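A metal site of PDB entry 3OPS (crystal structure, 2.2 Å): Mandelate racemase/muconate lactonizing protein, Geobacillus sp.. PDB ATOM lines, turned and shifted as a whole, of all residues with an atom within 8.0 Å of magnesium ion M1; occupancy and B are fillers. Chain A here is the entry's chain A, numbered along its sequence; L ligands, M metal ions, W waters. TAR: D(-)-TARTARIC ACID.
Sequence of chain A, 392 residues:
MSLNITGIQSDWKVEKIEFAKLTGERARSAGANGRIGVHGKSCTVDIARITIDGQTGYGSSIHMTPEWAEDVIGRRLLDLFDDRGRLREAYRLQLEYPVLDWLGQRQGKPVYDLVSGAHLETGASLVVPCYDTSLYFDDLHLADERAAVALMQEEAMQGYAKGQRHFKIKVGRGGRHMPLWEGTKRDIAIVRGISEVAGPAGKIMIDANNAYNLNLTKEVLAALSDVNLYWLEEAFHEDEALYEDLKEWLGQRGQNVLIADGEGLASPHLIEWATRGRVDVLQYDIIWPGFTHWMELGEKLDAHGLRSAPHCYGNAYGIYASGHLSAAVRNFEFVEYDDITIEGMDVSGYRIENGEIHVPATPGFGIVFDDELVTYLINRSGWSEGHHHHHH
The backbone NH (N) of Asn 210 lies within hydrogen-bond range of the backbone carbonyl oxygen (O) of Glu 234, 3.0 Å away. OE1 of Glu 238 sits at hydrogen-bond distance from N of Ser 267 (2.6 Å). O of Glu 234 is in hydrogen-bond range of N of Asn 209, at 3.5 Å. The side-chain carboxylate (OD2) of Asp 261 is in hydrogen-bond range of the side-chain hydroxyl (OH) of Tyr 243, 2.6 Å away. The backbone NH of Glu 234 is in hydrogen-bond range of the backbone carbonyl oxygen of Ala 260 (3.1 Å). The backbone carbonyl oxygen of Asp 261 lies within hydrogen-bond range of the backbone NH of Gln 283 (2.9 Å).
Water W1 lies within hydrogen-bond range of the backbone carbonyl oxygen of Glu 263 (2.9 Å), the side-chain carboxylate of Glu 238 (2.9 Å) and the backbone NH of Gly 262 (3.1 Å).
Within 4 Å of magnesium ion M1: Glu 234, Glu 238 and Asp 261. The nearest printed residue that does not touch magnesium ion M1 is Asn 210 (4.1 Å).
Magnesium ion M1 is bound by water W2 (2.0 Å), the side-chain carboxylate of Asp 261 (2.0 Å), the side-chain carboxylate of Glu 238 (2.1 Å), the side-chain carboxylate of Glu 234 (2.2 Å), water W1 (2.3 Å) and an oxygen (O41) of the ligand (2.5 Å).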
ATOM      1  N   ASN A 209      -3.786  26.355  14.774  1.00  0.00           N
ATOM      2  CA  ASN A 209      -4.172  27.197  15.899  1.00  0.00           C
ATOM      3  C   ASN A 209      -5.427  26.653  16.546  1.00  0.00           C
ATOM      4  O   ASN A 209      -6.433  27.362  16.683  1.00  0.00           O
ATOM      5  CB  ASN A 209      -4.295  28.669  15.483  1.00  0.00           C
ATOM      6  CG  ASN A 209      -2.943  29.330  15.238  1.00  0.00           C
ATOM      7  OD1 ASN A 209      -2.394  29.255  14.143  1.00  0.00           O
ATOM      8  ND2 ASN A 209      -2.400  29.970  16.279  1.00  0.00           N
ATOM      9  N   ASN A 210      -5.354  25.364  16.891  1.00  0.00           N
ATOM     10  CA  ASN A 210      -6.390  24.588  17.586  1.00  0.00           C
ATOM     11  C   ASN A 210      -7.733  24.357  16.865  1.00  0.00           C
ATOM     12  O   ASN A 210      -8.659  23.749  17.419  1.00  0.00           O
ATOM     13  CB  ASN A 210      -6.556  25.072  19.034  1.00  0.00           C
ATOM     14  CG  ASN A 210      -5.284  24.878  19.876  1.00  0.00           C
ATOM     15  OD1 ASN A 210      -4.500  23.955  19.628  1.00  0.00           O
ATOM     16  ND2 ASN A 210      -5.090  25.719  20.892  1.00  0.00           N
ATOM     17  N   GLU A 233       1.444  21.548  13.961  1.00  0.00           N
ATOM     18  CA  GLU A 233       1.429  22.368  15.156  1.00  0.00           C
ATOM     19  C   GLU A 233       0.016  22.679  15.648  1.00  0.00           C
ATOM     20  O   GLU A 233      -0.806  23.196  14.888  1.00  0.00           O
ATOM     21  CB  GLU A 233       2.194  23.661  14.913  1.00  0.00           C
ATOM     22  CG  GLU A 233       1.976  24.733  15.973  1.00  0.00           C
ATOM     23  CD  GLU A 233       2.931  25.882  15.818  1.00  0.00           C
ATOM     24  OE1 GLU A 233       3.826  25.746  14.966  1.00  0.00           O
ATOM     25  OE2 GLU A 233       2.795  26.907  16.533  1.00  0.00           O
ATOM     26  N   GLU A 234      -0.237  22.359  16.911  1.00  0.00           N
ATOM     27  CA  GLU A 234      -1.522  22.627  17.561  1.00  0.00           C
ATOM     28  C   GLU A 234      -2.715  22.304  16.657  1.00  0.00           C
ATOM     29  O   GLU A 234      -3.421  23.198  16.186  1.00  0.00           O
ATOM     30  CB  GLU A 234      -1.594  24.088  18.047  1.00  0.00           C
ATOM     31  CG  GLU A 234      -0.476  24.483  18.995  1.00  0.00           C
ATOM     32  CD  GLU A 234      -0.821  25.678  19.832  1.00  0.00           C
ATOM     33  OE1 GLU A 234      -1.214  26.716  19.243  1.00  0.00           O
ATOM     34  OE2 GLU A 234      -0.694  25.604  21.090  1.00  0.00           O
ATOM     35  N   ALA A 235      -2.921  21.012  16.417  1.00  0.00           N
ATOM     36  CA  ALA A 235      -4.100  20.536  15.702  1.00  0.00           C
ATOM     37  C   ALA A 235      -5.352  20.742  16.548  1.00  0.00           C
ATOM     38  O   ALA A 235      -6.446  20.984  16.037  1.00  0.00           O
ATOM     39  CB  ALA A 235      -3.935  19.065  15.350  1.00  0.00           C
ATOM     40  N   PHE A 236      -5.187  20.625  17.859  1.00  0.00           N
ATOM     41  CA  PHE A 236      -6.257  20.825  18.834  1.00  0.00           C
ATOM     42  C   PHE A 236      -5.504  21.072  20.114  1.00  0.00           C
ATOM     43  O   PHE A 236      -4.284  20.844  20.173  1.00  0.00           O
ATOM     44  CB  PHE A 236      -7.159  19.583  18.954  1.00  0.00           C
ATOM     45  CG  PHE A 236      -6.428  18.274  18.740  1.00  0.00           C
ATOM     46  CD1 PHE A 236      -6.294  17.731  17.453  1.00  0.00           C
ATOM     47  CD2 PHE A 236      -5.875  17.590  19.813  1.00  0.00           C
ATOM     48  CE1 PHE A 236      -5.621  16.535  17.254  1.00  0.00           C
ATOM     49  CE2 PHE A 236      -5.205  16.390  19.605  1.00  0.00           C
ATOM     50  CZ  PHE A 236      -5.065  15.869  18.329  1.00  0.00           C
ATOM     51  N   HIS A 237      -6.166  21.565  21.145  1.00  0.00           N
ATOM     52  CA  HIS A 237      -5.446  21.763  22.391  1.00  0.00           C
ATOM     53  C   HIS A 237      -4.869  20.418  22.853  1.00  0.00           C
ATOM     54  O   HIS A 237      -5.480  19.367  22.674  1.00  0.00           O
ATOM     55  CB  HIS A 237      -6.275  22.434  23.473  1.00  0.00           C
ATOM     56  CG  HIS A 237      -5.453  22.935  24.635  1.00  0.00           C
ATOM     57  ND1 HIS A 237      -4.935  22.096  25.597  1.00  0.00           N
ATOM     58  CD2 HIS A 237      -5.042  24.169  24.960  1.00  0.00           C
ATOM     59  CE1 HIS A 237      -4.263  22.807  26.490  1.00  0.00           C
ATOM     60  NE2 HIS A 237      -4.316  24.071  26.124  1.00  0.00           N
ATOM     61  N   GLU A 238      -3.662  20.487  23.413  1.00  0.00           N
ATOM     62  CA  GLU A 238      -2.870  19.296  23.710  1.00  0.00           C
ATOM     63  C   GLU A 238      -3.556  18.402  24.723  1.00  0.00           C
ATOM     64  O   GLU A 238      -3.977  18.826  25.794  1.00  0.00           O
ATOM     65  CB  GLU A 238      -1.445  19.681  24.130  1.00  0.00           C
ATOM     66  CG  GLU A 238      -1.353  20.593  25.343  1.00  0.00           C
ATOM     67  CD  GLU A 238      -1.241  22.077  24.991  1.00  0.00           C
ATOM     68  OE1 GLU A 238      -0.876  22.866  25.889  1.00  0.00           O
ATOM     69  OE2 GLU A 238      -1.508  22.472  23.834  1.00  0.00           O
ATOM     70  N   ASP A 239      -3.674  17.128  24.343  1.00  0.00           N
ATOM     71  CA  ASP A 239      -4.337  16.125  25.138  1.00  0.00           C
ATOM     72  C   ASP A 239      -3.574  14.855  24.855  1.00  0.00           C
ATOM     73  O   ASP A 239      -3.500  14.434  23.699  1.00  0.00           O
ATOM     74  CB  ASP A 239      -5.824  16.004  24.719  1.00  0.00           C
ATOM     75  CG  ASP A 239      -6.512  14.759  25.287  1.00  0.00           C
ATOM     76  OD1 ASP A 239      -5.801  13.788  25.628  1.00  0.00           O
ATOM     77  OD2 ASP A 239      -7.772  14.724  25.387  1.00  0.00           O
ATOM     78  N   TYR A 243      -3.208  12.656  21.280  1.00  0.00           N
ATOM     79  CA  TYR A 243      -1.877  12.586  20.631  1.00  0.00           C
ATOM     80  C   TYR A 243      -1.300  11.174  20.651  1.00  0.00           C
ATOM     81  O   TYR A 243      -0.538  10.806  19.755  1.00  0.00           O
ATOM     82  CB  TYR A 243      -0.876  13.530  21.297  1.00  0.00           C
ATOM     83  CG  TYR A 243      -0.946  14.983  20.868  1.00  0.00           C
ATOM     84  CD1 TYR A 243      -1.298  15.353  19.569  1.00  0.00           C
ATOM     85  CD2 TYR A 243      -0.609  15.983  21.770  1.00  0.00           C
ATOM     86  CE1 TYR A 243      -1.341  16.698  19.207  1.00  0.00           C
ATOM     87  CE2 TYR A 243      -0.638  17.313  21.408  1.00  0.00           C
ATOM     88  CZ  TYR A 243      -1.005  17.670  20.134  1.00  0.00           C
ATOM     89  OH  TYR A 243      -1.033  19.004  19.795  1.00  0.00           O
ATOM     90  N   ALA A 260       4.139  19.253  17.193  1.00  0.00           N
ATOM     91  CA  ALA A 260       4.630  20.441  17.877  1.00  0.00           C
ATOM     92  C   ALA A 260       3.511  21.135  18.629  1.00  0.00           C
ATOM     93  O   ALA A 260       2.374  21.156  18.150  1.00  0.00           O
ATOM     94  CB  ALA A 260       5.257  21.391  16.873  1.00  0.00           C
ATOM     95  N   ASP A 261       3.820  21.682  19.801  1.00  0.00           N
ATOM     96  CA  ASP A 261       2.825  22.323  20.659  1.00  0.00           C
ATOM     97  C   ASP A 261       3.516  23.102  21.796  1.00  0.00           C
ATOM     98  O   ASP A 261       4.729  23.042  21.930  1.00  0.00           O
ATOM     99  CB  ASP A 261       1.861  21.271  21.222  1.00  0.00           C
ATOM    100  CG  ASP A 261       0.462  21.828  21.467  1.00  0.00           C
ATOM    101  OD1 ASP A 261       0.333  23.025  21.833  1.00  0.00           O
ATOM    102  OD2 ASP A 261      -0.512  21.081  21.300  1.00  0.00           O
ATOM    103  N   GLY A 262       2.758  23.860  22.604  1.00  0.00           N
ATOM    104  CA  GLY A 262       3.390  24.593  23.717  1.00  0.00           C
ATOM    105  C   GLY A 262       3.138  26.087  23.880  1.00  0.00           C
ATOM    106  O   GLY A 262       3.064  26.564  25.019  1.00  0.00           O
ATOM    107  N   GLU A 263       3.025  26.822  22.777  1.00  0.00           N
ATOM    108  CA  GLU A 263       2.713  28.260  22.814  1.00  0.00           C
ATOM    109  C   GLU A 263       1.402  28.526  23.560  1.00  0.00           C
ATOM    110  O   GLU A 263       0.664  27.603  23.870  1.00  0.00           O
ATOM    111  CB  GLU A 263       2.643  28.826  21.396  1.00  0.00           C
ATOM    112  CG  GLU A 263       1.345  28.541  20.671  1.00  0.00           C
ATOM    113  CD  GLU A 263       1.248  29.226  19.312  1.00  0.00           C
ATOM    114  OE1 GLU A 263       0.548  30.257  19.212  1.00  0.00           O
ATOM    115  OE2 GLU A 263       1.846  28.731  18.333  1.00  0.00           O
ATOM    116  N   GLY A 264       1.133  29.803  23.848  1.00  0.00           N
ATOM    117  CA  GLY A 264      -0.125  30.211  24.490  1.00  0.00           C
ATOM    118  C   GLY A 264      -0.198  29.731  25.924  1.00  0.00           C
ATOM    119  O   GLY A 264       0.835  29.582  26.593  1.00  0.00           O
ATOM    120  N   LEU A 265      -1.422  29.465  26.361  1.00  0.00           N
ATOM    121  CA  LEU A 265      -1.716  28.896  27.669  1.00  0.00           C
ATOM    122  C   LEU A 265      -1.546  27.401  27.613  1.00  0.00           C
ATOM    123  O   LEU A 265      -2.487  26.666  27.367  1.00  0.00           O
ATOM    124  CB  LEU A 265      -3.151  29.220  28.056  1.00  0.00           C
ATOM    125  CG  LEU A 265      -3.468  30.693  28.066  1.00  0.00           C
ATOM    126  CD1 LEU A 265      -4.875  30.973  27.642  1.00  0.00           C
ATOM    127  CD2 LEU A 265      -3.163  31.306  29.398  1.00  0.00           C
ATOM    128  N   ALA A 266      -0.326  26.950  27.865  1.00  0.00           N
ATOM    129  CA  ALA A 266       0.008  25.539  27.735  1.00  0.00           C
ATOM    130  C   ALA A 266      -0.640  24.688  28.818  1.00  0.00           C
ATOM    131  O   ALA A 266      -0.840  25.139  29.951  1.00  0.00           O
ATOM    132  CB  ALA A 266       1.503  25.384  27.799  1.00  0.00           C
ATOM    133  N   SER A 267      -0.933  23.441  28.449  1.00  0.00           N
ATOM    134  CA  SER A 267      -1.156  22.394  29.429  1.00  0.00           C
ATOM    135  C   SER A 267       0.060  22.306  30.337  1.00  0.00           C
ATOM    136  O   SER A 267       1.196  22.102  29.860  1.00  0.00           O
ATOM    137  CB  SER A 267      -1.344  21.052  28.731  1.00  0.00           C
ATOM    138  OG  SER A 267      -1.192  19.989  29.646  1.00  0.00           O
ATOM    139  N   LEU A 270       2.319  19.357  29.705  1.00  0.00           N
ATOM    140  CA  LEU A 270       2.841  19.217  28.344  1.00  0.00           C
ATOM    141  C   LEU A 270       4.207  18.525  28.215  1.00  0.00           C
ATOM    142  O   LEU A 270       4.409  17.731  27.299  1.00  0.00           O
ATOM    143  CB  LEU A 270       2.882  20.573  27.644  1.00  0.00           C
ATOM    144  CG  LEU A 270       3.191  20.592  26.149  1.00  0.00           C
ATOM    145  CD1 LEU A 270       2.409  19.504  25.381  1.00  0.00           C
ATOM    146  CD2 LEU A 270       2.891  21.935  25.597  1.00  0.00           C
ATOM    147  N   GLN A 283       7.295  24.296  22.209  1.00  0.00           N
ATOM    148  CA  GLN A 283       7.129  25.607  21.557  1.00  0.00           C
ATOM    149  C   GLN A 283       6.782  26.763  22.462  1.00  0.00           C
ATOM    150  O   GLN A 283       5.961  27.625  22.102  1.00  0.00           O
ATOM    151  CB  GLN A 283       6.072  25.538  20.446  1.00  0.00           C
ATOM    152  CG  GLN A 283       6.359  24.562  19.382  1.00  0.00           C
ATOM    153  CD  GLN A 283       5.420  24.718  18.218  1.00  0.00           C
ATOM    154  OE1 GLN A 283       4.217  24.560  18.367  1.00  0.00           O
ATOM    155  NE2 GLN A 283       5.967  25.041  17.057  1.00  0.00           N
HETATM  156  O1  TAR L   1      -6.604  28.414  25.031  1.00  0.00           O
HETATM  157  O11 TAR L   1      -6.366  27.157  23.245  1.00  0.00           O
HETATM  158  C1  TAR L   1      -5.964  27.579  24.357  1.00  0.00           C
HETATM  159  C2  TAR L   1      -4.683  27.005  24.920  1.00  0.00           C
HETATM  160  O2  TAR L   1      -4.741  27.059  26.357  1.00  0.00           O
HETATM  161  C3  TAR L   1      -3.387  27.661  24.438  1.00  0.00           C
HETATM  162  O3  TAR L   1      -3.535  29.091  24.303  1.00  0.00           O
HETATM  163  C4  TAR L   1      -2.811  27.036  23.187  1.00  0.00           C
HETATM  164  O4  TAR L   1      -2.119  27.776  22.427  1.00  0.00           O
HETATM  165  O41 TAR L   1      -3.008  25.796  22.954  1.00  0.00           O
HETATM  166 MG    MG M   1      -1.419  23.948  22.353  1.00  0.00          MG
HETATM  167 MG    MG M   2       1.285  28.321  16.567  1.00  0.00          MG
HETATM  168  O   HOH W   1       0.092  24.785  23.942  1.00  0.00           O
HETATM  169  O   HOH W   2      -2.500  22.631  21.370  1.00  0.00           O
